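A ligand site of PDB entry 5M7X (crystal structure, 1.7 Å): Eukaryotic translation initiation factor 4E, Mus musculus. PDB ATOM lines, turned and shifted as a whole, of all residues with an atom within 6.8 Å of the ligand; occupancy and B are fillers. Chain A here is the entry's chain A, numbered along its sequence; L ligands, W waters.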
ATOM      1  N   PHE A  21      11.685   0.779   6.651  1.00  0.00           N
ATOM      2  CA  PHE A  21      12.141  -0.539   6.218  1.00  0.00           C
ATOM      3  C   PHE A  21      12.107  -1.467   7.426  1.00  0.00           C
ATOM      4  O   PHE A  21      12.643  -1.131   8.481  1.00  0.00           O
ATOM      5  CB  PHE A  21      13.564  -0.452   5.658  1.00  0.00           C
ATOM      6  CG  PHE A  21      14.148  -1.778   5.270  1.00  0.00           C
ATOM      7  CD1 PHE A  21      14.788  -2.569   6.199  1.00  0.00           C
ATOM      8  CD2 PHE A  21      14.057  -2.209   3.960  1.00  0.00           C
ATOM      9  CE1 PHE A  21      15.303  -3.802   5.836  1.00  0.00           C
ATOM     10  CE2 PHE A  21      14.591  -3.423   3.591  1.00  0.00           C
ATOM     11  CZ  PHE A  21      15.204  -4.224   4.533  1.00  0.00           C
ATOM     12  N   TRP A  29      14.484  -7.054  -0.572  1.00  0.00           N
ATOM     13  CA  TRP A  29      14.814  -5.774   0.073  1.00  0.00           C
ATOM     14  C   TRP A  29      13.827  -4.687  -0.364  1.00  0.00           C
ATOM     15  O   TRP A  29      13.289  -3.949   0.454  1.00  0.00           O
ATOM     16  CB  TRP A  29      16.254  -5.358  -0.244  1.00  0.00           C
ATOM     17  CG  TRP A  29      16.627  -4.069   0.438  1.00  0.00           C
ATOM     18  CD1 TRP A  29      17.119  -3.926   1.716  1.00  0.00           C
ATOM     19  CD2 TRP A  29      16.522  -2.730  -0.097  1.00  0.00           C
ATOM     20  NE1 TRP A  29      17.329  -2.607   1.994  1.00  0.00           N
ATOM     21  CE2 TRP A  29      16.958  -1.846   0.910  1.00  0.00           C
ATOM     22  CE3 TRP A  29      16.085  -2.214  -1.319  1.00  0.00           C
ATOM     23  CZ2 TRP A  29      16.987  -0.464   0.731  1.00  0.00           C
ATOM     24  CZ3 TRP A  29      16.115  -0.832  -1.498  1.00  0.00           C
ATOM     25  CH2 TRP A  29      16.567   0.029  -0.483  1.00  0.00           C
ATOM     26  N   GLN A  30      13.550  -4.604  -1.671  1.00  0.00           N
ATOM     27  CA  GLN A  30      12.668  -3.537  -2.147  1.00  0.00           C
ATOM     28  C   GLN A  30      11.258  -3.696  -1.588  1.00  0.00           C
ATOM     29  O   GLN A  30      10.596  -2.696  -1.280  1.00  0.00           O
ATOM     30  CB  GLN A  30      12.629  -3.522  -3.671  1.00  0.00           C
ATOM     31  CG  GLN A  30      13.920  -3.059  -4.327  1.00  0.00           C
ATOM     32  N   GLY A  61      17.387  -4.126  12.605  1.00  0.00           N
ATOM     33  CA  GLY A  61      17.091  -4.425  11.218  1.00  0.00           C
ATOM     34  C   GLY A  61      16.163  -3.445  10.525  1.00  0.00           C
ATOM     35  O   GLY A  61      15.895  -3.630   9.324  1.00  0.00           O
ATOM     36  N   ASP A  63      14.985   0.536   9.211  1.00  0.00           N
ATOM     37  CA  ASP A  63      15.497   1.848   8.786  1.00  0.00           C
ATOM     38  C   ASP A  63      14.379   2.876   8.756  1.00  0.00           C
ATOM     39  O   ASP A  63      13.209   2.562   8.507  1.00  0.00           O
ATOM     40  CB  ASP A  63      16.096   1.867   7.369  1.00  0.00           C
ATOM     41  CG  ASP A  63      16.975   0.699   7.054  1.00  0.00           C
ATOM     42  OD1 ASP A  63      17.680   0.216   7.952  1.00  0.00           O
ATOM     43  OD2 ASP A  63      16.996   0.307   5.868  1.00  0.00           O
ATOM     44  N   PRO A  73      14.406   5.968  -1.774  1.00  0.00           N
ATOM     45  CA  PRO A  73      15.624   5.794  -0.981  1.00  0.00           C
ATOM     46  C   PRO A  73      16.401   4.545  -1.363  1.00  0.00           C
ATOM     47  O   PRO A  73      16.668   3.660  -0.542  1.00  0.00           O
ATOM     48  CB  PRO A  73      15.078   5.688   0.446  1.00  0.00           C
ATOM     49  CG  PRO A  73      13.694   5.229   0.338  1.00  0.00           C
ATOM     50  CD  PRO A  73      13.179   5.560  -1.059  1.00  0.00           C
ATOM     51  N   MET A  74      16.760   4.452  -2.641  1.00  0.00           N
ATOM     52  CA  MET A  74      17.495   3.292  -3.096  1.00  0.00           C
ATOM     53  C   MET A  74      18.490   3.722  -4.156  1.00  0.00           C
ATOM     54  O   MET A  74      18.290   4.730  -4.845  1.00  0.00           O
ATOM     55  CB  MET A  74      16.567   2.204  -3.660  1.00  0.00           C
ATOM     56  CG  MET A  74      15.851   2.595  -4.921  1.00  0.00           C
ATOM     57  SD  MET A  74      14.675   1.302  -5.386  1.00  0.00           S
ATOM     58  CE  MET A  74      13.450   1.398  -4.111  1.00  0.00           C
ATOM     59  N   TRP A  75      19.586   2.973  -4.234  1.00  0.00           N
ATOM     60  CA  TRP A  75      20.658   3.293  -5.176  1.00  0.00           C
ATOM     61  C   TRP A  75      20.156   3.425  -6.605  1.00  0.00           C
ATOM     62  O   TRP A  75      20.717   4.193  -7.394  1.00  0.00           O
ATOM     63  CB  TRP A  75      21.740   2.211  -5.174  1.00  0.00           C
ATOM     64  CG  TRP A  75      22.284   1.821  -3.852  1.00  0.00           C
ATOM     65  CD1 TRP A  75      22.605   2.645  -2.809  1.00  0.00           C
ATOM     66  CD2 TRP A  75      22.609   0.489  -3.436  1.00  0.00           C
ATOM     67  NE1 TRP A  75      23.088   1.905  -1.769  1.00  0.00           N
ATOM     68  CE2 TRP A  75      23.108   0.585  -2.127  1.00  0.00           C
ATOM     69  CE3 TRP A  75      22.515  -0.764  -4.042  1.00  0.00           C
ATOM     70  CZ2 TRP A  75      23.521  -0.537  -1.407  1.00  0.00           C
ATOM     71  CZ3 TRP A  75      22.928  -1.886  -3.322  1.00  0.00           C
ATOM     72  CH2 TRP A  75      23.416  -1.760  -2.011  1.00  0.00           C
ATOM     73  N   GLU A  76      19.125   2.645  -6.981  1.00  0.00           N
ATOM     74  CA  GLU A  76      18.664   2.552  -8.369  1.00  0.00           C
ATOM     75  C   GLU A  76      17.927   3.796  -8.859  1.00  0.00           C
ATOM     76  O   GLU A  76      17.725   3.925 -10.069  1.00  0.00           O
ATOM     77  CB  GLU A  76      17.803   1.315  -8.562  1.00  0.00           C
ATOM     78  CG  GLU A  76      18.591   0.016  -8.380  1.00  0.00           C
ATOM     79  CD  GLU A  76      18.521  -0.548  -6.985  1.00  0.00           C
ATOM     80  OE1 GLU A  76      18.530  -1.790  -6.853  1.00  0.00           O
ATOM     81  OE2 GLU A  76      18.518   0.243  -6.017  1.00  0.00           O
ATOM     82  N   ARG A  85      27.112   8.839  -0.240  1.00  0.00           N
ATOM     83  CA  ARG A  85      26.621   9.134   1.100  1.00  0.00           C
ATOM     84  C   ARG A  85      27.766   9.543   2.025  1.00  0.00           C
ATOM     85  O   ARG A  85      28.852   8.947   2.000  1.00  0.00           O
ATOM     86  CB  ARG A  85      25.867   7.939   1.696  1.00  0.00           C
ATOM     87  CG  ARG A  85      26.723   6.697   1.924  1.00  0.00           C
ATOM     88  CD  ARG A  85      25.947   5.621   2.653  1.00  0.00           C
ATOM     89  NE  ARG A  85      26.775   4.434   2.875  1.00  0.00           N
ATOM     90  CZ  ARG A  85      26.350   3.326   3.474  1.00  0.00           C
ATOM     91  NH1 ARG A  85      25.104   3.254   3.942  1.00  0.00           N
ATOM     92  NH2 ARG A  85      27.176   2.287   3.616  1.00  0.00           N
ATOM     93  N   VAL A 126      19.306   8.503   5.665  1.00  0.00           N
ATOM     94  CA  VAL A 126      18.912   7.160   6.099  1.00  0.00           C
ATOM     95  C   VAL A 126      19.507   6.901   7.458  1.00  0.00           C
ATOM     96  O   VAL A 126      20.686   7.169   7.679  1.00  0.00           O
ATOM     97  CB  VAL A 126      19.417   6.089   5.116  1.00  0.00           C
ATOM     98  CG1 VAL A 126      19.071   4.689   5.615  1.00  0.00           C
ATOM     99  CG2 VAL A 126      18.841   6.326   3.706  1.00  0.00           C
ATOM    100  N   ASN A 128      20.019   3.468   9.825  1.00  0.00           N
ATOM    101  CA  ASN A 128      19.947   2.020   9.942  1.00  0.00           C
ATOM    102  C   ASN A 128      20.112   1.650  11.406  1.00  0.00           C
ATOM    103  O   ASN A 128      21.160   1.937  11.995  1.00  0.00           O
ATOM    104  CB  ASN A 128      21.016   1.329   9.101  1.00  0.00           C
ATOM    105  CG  ASN A 128      21.058   1.831   7.671  1.00  0.00           C
ATOM    106  OD1 ASN A 128      20.178   1.502   6.864  1.00  0.00           O
ATOM    107  ND2 ASN A 128      22.177   2.445   7.297  1.00  0.00           N
ATOM    108  N   VAL A 129      19.114   0.987  11.982  1.00  0.00           N
ATOM    109  CA  VAL A 129      19.222   0.476  13.351  1.00  0.00           C
ATOM    110  C   VAL A 129      19.656  -0.976  13.248  1.00  0.00           C
ATOM    111  O   VAL A 129      18.916  -1.808  12.711  1.00  0.00           O
ATOM    112  CB  VAL A 129      17.885   0.621  14.105  1.00  0.00           C
ATOM    113  CG1 VAL A 129      18.029   0.155  15.546  1.00  0.00           C
ATOM    114  CG2 VAL A 129      17.426   2.074  14.058  1.00  0.00           C
ATOM    115  N   ARG A 130      20.851  -1.266  13.759  1.00  0.00           N
ATOM    116  CA  ARG A 130      21.409  -2.616  13.659  1.00  0.00           C
ATOM    117  C   ARG A 130      22.121  -3.010  14.934  1.00  0.00           C
ATOM    118  O   ARG A 130      22.753  -2.197  15.607  1.00  0.00           O
ATOM    119  CB  ARG A 130      22.406  -2.760  12.508  1.00  0.00           C
ATOM    120  CG  ARG A 130      21.963  -2.215  11.192  1.00  0.00           C
ATOM    121  CD  ARG A 130      21.102  -3.269  10.588  1.00  0.00           C
ATOM    122  NE  ARG A 130      20.801  -2.952   9.186  1.00  0.00           N
ATOM    123  CZ  ARG A 130      19.749  -2.224   8.839  1.00  0.00           C
ATOM    124  NH1 ARG A 130      18.951  -1.705   9.771  1.00  0.00           N
ATOM    125  NH2 ARG A 130      19.525  -1.977   7.553  1.00  0.00           N
ATOM    126  N   GLY A 133      25.837  -2.184  15.214  1.00  0.00           N
ATOM    127  CA  GLY A 133      26.214  -0.779  15.258  1.00  0.00           C
ATOM    128  C   GLY A 133      25.326   0.012  14.312  1.00  0.00           C
ATOM    129  O   GLY A 133      25.201  -0.340  13.133  1.00  0.00           O
ATOM    130  N   ASP A 134      24.744   1.109  14.773  1.00  0.00           N
ATOM    131  CA  ASP A 134      23.835   1.866  13.913  1.00  0.00           C
ATOM    132  C   ASP A 134      24.602   2.759  12.924  1.00  0.00           C
ATOM    133  O   ASP A 134      25.807   2.990  13.064  1.00  0.00           O
ATOM    134  CB  ASP A 134      22.890   2.729  14.762  1.00  0.00           C
ATOM    135  CG  ASP A 134      22.192   1.941  15.866  1.00  0.00           C
ATOM    136  OD1 ASP A 134      21.638   0.854  15.575  1.00  0.00           O
ATOM    137  OD2 ASP A 134      22.202   2.398  17.028  1.00  0.00           O
ATOM    138  N   LYS A 135      23.894   3.207  11.892  1.00  0.00           N
ATOM    139  CA  LYS A 135      24.461   4.128  10.891  1.00  0.00           C
ATOM    140  C   LYS A 135      23.452   5.227  10.562  1.00  0.00           C
ATOM    141  O   LYS A 135      22.246   4.976  10.522  1.00  0.00           O
ATOM    142  CB  LYS A 135      24.858   3.404   9.583  1.00  0.00           C
ATOM    143  CG  LYS A 135      25.920   2.311   9.757  1.00  0.00           C
ATOM    144  CD  LYS A 135      26.210   1.622   8.422  1.00  0.00           C
ATOM    145  CE  LYS A 135      27.075   0.370   8.643  1.00  0.00           C
ATOM    146  NZ  LYS A 135      27.658  -0.140   7.377  1.00  0.00           N
ATOM    147  N   TRP A 139      22.582  11.254   1.809  1.00  0.00           N
ATOM    148  CA  TRP A 139      22.795  10.844   0.431  1.00  0.00           C
ATOM    149  C   TRP A 139      22.775  12.066  -0.480  1.00  0.00           C
ATOM    150  O   TRP A 139      21.886  12.923  -0.350  1.00  0.00           O
ATOM    151  CB  TRP A 139      21.703   9.870  -0.028  1.00  0.00           C
ATOM    152  CG  TRP A 139      21.735   8.486   0.559  1.00  0.00           C
ATOM    153  CD1 TRP A 139      22.252   8.099   1.768  1.00  0.00           C
ATOM    154  CD2 TRP A 139      21.241   7.297  -0.068  1.00  0.00           C
ATOM    155  NE1 TRP A 139      22.079   6.730   1.936  1.00  0.00           N
ATOM    156  CE2 TRP A 139      21.480   6.217   0.816  1.00  0.00           C
ATOM    157  CE3 TRP A 139      20.610   7.052  -1.294  1.00  0.00           C
ATOM    158  CZ2 TRP A 139      21.095   4.916   0.509  1.00  0.00           C
ATOM    159  CZ3 TRP A 139      20.238   5.749  -1.596  1.00  0.00           C
ATOM    160  CH2 TRP A 139      20.484   4.697  -0.698  1.00  0.00           C
ATOM    161  N   HIS A 173      27.649   5.150  -4.036  1.00  0.00           N
ATOM    162  CA  HIS A 173      26.748   4.003  -4.046  1.00  0.00           C
ATOM    163  C   HIS A 173      27.208   2.921  -5.007  1.00  0.00           C
ATOM    164  O   HIS A 173      26.964   1.728  -4.771  1.00  0.00           O
ATOM    165  CB  HIS A 173      25.320   4.414  -4.413  1.00  0.00           C
ATOM    166  CG  HIS A 173      24.701   5.411  -3.478  1.00  0.00           C
ATOM    167  ND1 HIS A 173      24.702   5.257  -2.118  1.00  0.00           N
ATOM    168  CD2 HIS A 173      24.059   6.581  -3.735  1.00  0.00           C
ATOM    169  CE1 HIS A 173      24.084   6.296  -1.558  1.00  0.00           C
ATOM    170  NE2 HIS A 173      23.685   7.107  -2.522  1.00  0.00           N
ATOM    171  N   THR A 176      29.355   0.820  -3.069  1.00  0.00           N
ATOM    172  CA  THR A 176      28.586   0.053  -2.096  1.00  0.00           C
ATOM    173  C   THR A 176      27.851  -1.114  -2.749  1.00  0.00           C
ATOM    174  O   THR A 176      27.793  -2.211  -2.185  1.00  0.00           O
ATOM    175  CB  THR A 176      27.591   0.977  -1.380  1.00  0.00           C
ATOM    176  OG1 THR A 176      28.275   2.138  -0.886  1.00  0.00           O
ATOM    177  CG2 THR A 176      26.936   0.255  -0.214  1.00  0.00           C
HETATM  178  O1  LIG L   1      22.370  -0.922   4.021  1.00  0.00           O
HETATM  179  P1  LIG L   1      22.097  -2.348   4.463  1.00  0.00           P
HETATM  180  O2  LIG L   1      20.847  -2.670   5.223  1.00  0.00           O
HETATM  181  O3  LIG L   1      23.418  -2.904   5.192  1.00  0.00           O
HETATM  182  P2  LIG L   1      23.622  -3.046   6.781  1.00  0.00           P
HETATM  183  O4  LIG L   1      22.532  -3.864   7.348  1.00  0.00           O
HETATM  184 SE1  LIG L   1      23.733  -1.205   7.772  1.00  0.00          SE
HETATM  185  O5  LIG L   1      24.994  -3.879   6.916  1.00  0.00           O
HETATM  186  P3  LIG L   1      26.350  -3.680   6.070  1.00  0.00           P
HETATM  187  O6  LIG L   1      26.444  -4.987   5.302  1.00  0.00           O
HETATM  188  O7  LIG L   1      26.151  -2.470   5.184  1.00  0.00           O
HETATM  189  O8  LIG L   1      27.453  -3.506   7.219  1.00  0.00           O
HETATM  190  O9  LIG L   1      22.172  -3.258   3.136  1.00  0.00           O
HETATM  191  C1  LIG L   1      22.098  -4.679   3.272  1.00  0.00           C
HETATM  192  C2  LIG L   1      21.610  -5.199   1.938  1.00  0.00           C
HETATM  193  C3  LIG L   1      22.499  -4.814   0.785  1.00  0.00           C
HETATM  194  O10 LIG L   1      23.564  -5.750   0.680  1.00  0.00           O
HETATM  195  C4  LIG L   1      21.548  -4.926  -0.374  1.00  0.00           C
HETATM  196  O11 LIG L   1      21.425  -6.295  -0.746  1.00  0.00           O
HETATM  197  C5  LIG L   1      20.731  -6.472  -1.979  1.00  0.00           C
HETATM  198  C6  LIG L   1      20.246  -4.428   0.235  1.00  0.00           C
HETATM  199  O12 LIG L   1      20.364  -4.600   1.644  1.00  0.00           O
HETATM  200  N1  LIG L   1      20.154  -2.984  -0.060  1.00  0.00           N
HETATM  201  C7  LIG L   1      19.795  -2.517  -1.267  1.00  0.00           C
HETATM  202  N2  LIG L   1      19.425  -3.149  -2.390  1.00  0.00           N
HETATM  203  C8  LIG L   1      19.088  -2.421  -3.477  1.00  0.00           C
HETATM  204  N3  LIG L   1      18.727  -3.052  -4.604  1.00  0.00           N
HETATM  205  N4  LIG L   1      19.120  -1.061  -3.441  1.00  0.00           N
HETATM  206  C9  LIG L   1      19.478  -0.408  -2.319  1.00  0.00           C
HETATM  207  O13 LIG L   1      19.503   0.942  -2.339  1.00  0.00           O
HETATM  208  C10 LIG L   1      19.842  -1.154  -1.204  1.00  0.00           C
HETATM  209  N5  LIG L   1      20.235  -0.781   0.031  1.00  0.00           N
HETATM  210  C11 LIG L   1      20.428   0.590   0.575  1.00  0.00           C
HETATM  211  C12 LIG L   1      20.449  -1.926   0.738  1.00  0.00           C
HETATM  212  O   HOH W   1      18.447  -1.269   4.294  1.00  0.00           O
HETATM  213  O   HOH W   2      23.384   1.171   5.160  1.00  0.00           O
HETATM  214  O   HOH W   3      18.956  -4.452   5.278  1.00  0.00           O
HETATM  215  O   HOH W   4      25.737  -2.819   1.952  1.00  0.00           O
HETATM  216  O   HOH W   5      26.153  -0.030   4.932  1.00  0.00           O
HETATM  217  O   HOH W   6      24.258  -0.475   2.069  1.00  0.00           O
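Water W5 lies within hydrogen-bond range of O7 of the ligand (2.5 Å), NH2 of Arg 85 (2.9 Å) and NZ of Lys 135 (2.9 Å). Water W2 lies within hydrogen-bond range of an oxygen (O1) of the ligand (2.6 Å), the side-chain amide nitrogen (ND2) of Asn 128 (2.8 Å) and the guanidinium group (NH1) of Arg 85 (3.0 Å). Water W3 bridges O2 of the ligand (2.6 Å) and NH2 of Arg 130 (3.4 Å). Water W1 lies within hydrogen-bond range of the side-chain carboxylate of Asp 63 (2.7 Å), the indole nitrogen of Trp 29 (2.9 Å) and an oxygen (O2) of the ligand (2.9 Å).
Trp 29 touches the ligand (CD1 to O12, 3.3 Å). Met 74 touches the ligand. CB of Asn 128 touches SE1 of the ligand (3.9 Å). Seven residues have an atom within 4 Å of the ligand: Trp 29, Met 74, Trp 75, Glu 76, Asn 128, Arg 130 and Lys 135. The nearest printed residue that does not touch the ligand is Trp 139 (4.2 Å).
NH2 of Arg 130 is in salt-bridge range of OD1 of Asp 63 (2.9 Å). The backbone NH (N) of Arg 130 is in hydrogen-bond range of the side-chain carboxylate (OD1) of Asp 134, 2.9 Å away. The backbone NH (N) of Asn 128 lies within hydrogen-bond range of the backbone carbonyl oxygen (O) of Lys 135, at 2.8 Å. OD1 of Asn 128 lies close to OD1 of Asp 63, 3.0 Å away.
A nitrogen (N3) of the ligand sits at hydrogen-bond distance from the side-chain carboxylate (OE1) of Glu 76, at 2.6 Å. NH2 of Arg 130 lies within salt-bridge range of O2 of the ligand, at 2.8 Å. An oxygen (O13) of the ligand is in hydrogen-bond range of the backbone NH (N) of Trp 75. The side-chain amino group (NZ) of Lys 135 lies within salt-bridge range of an oxygen (O8) of the ligand (3.4 Å).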
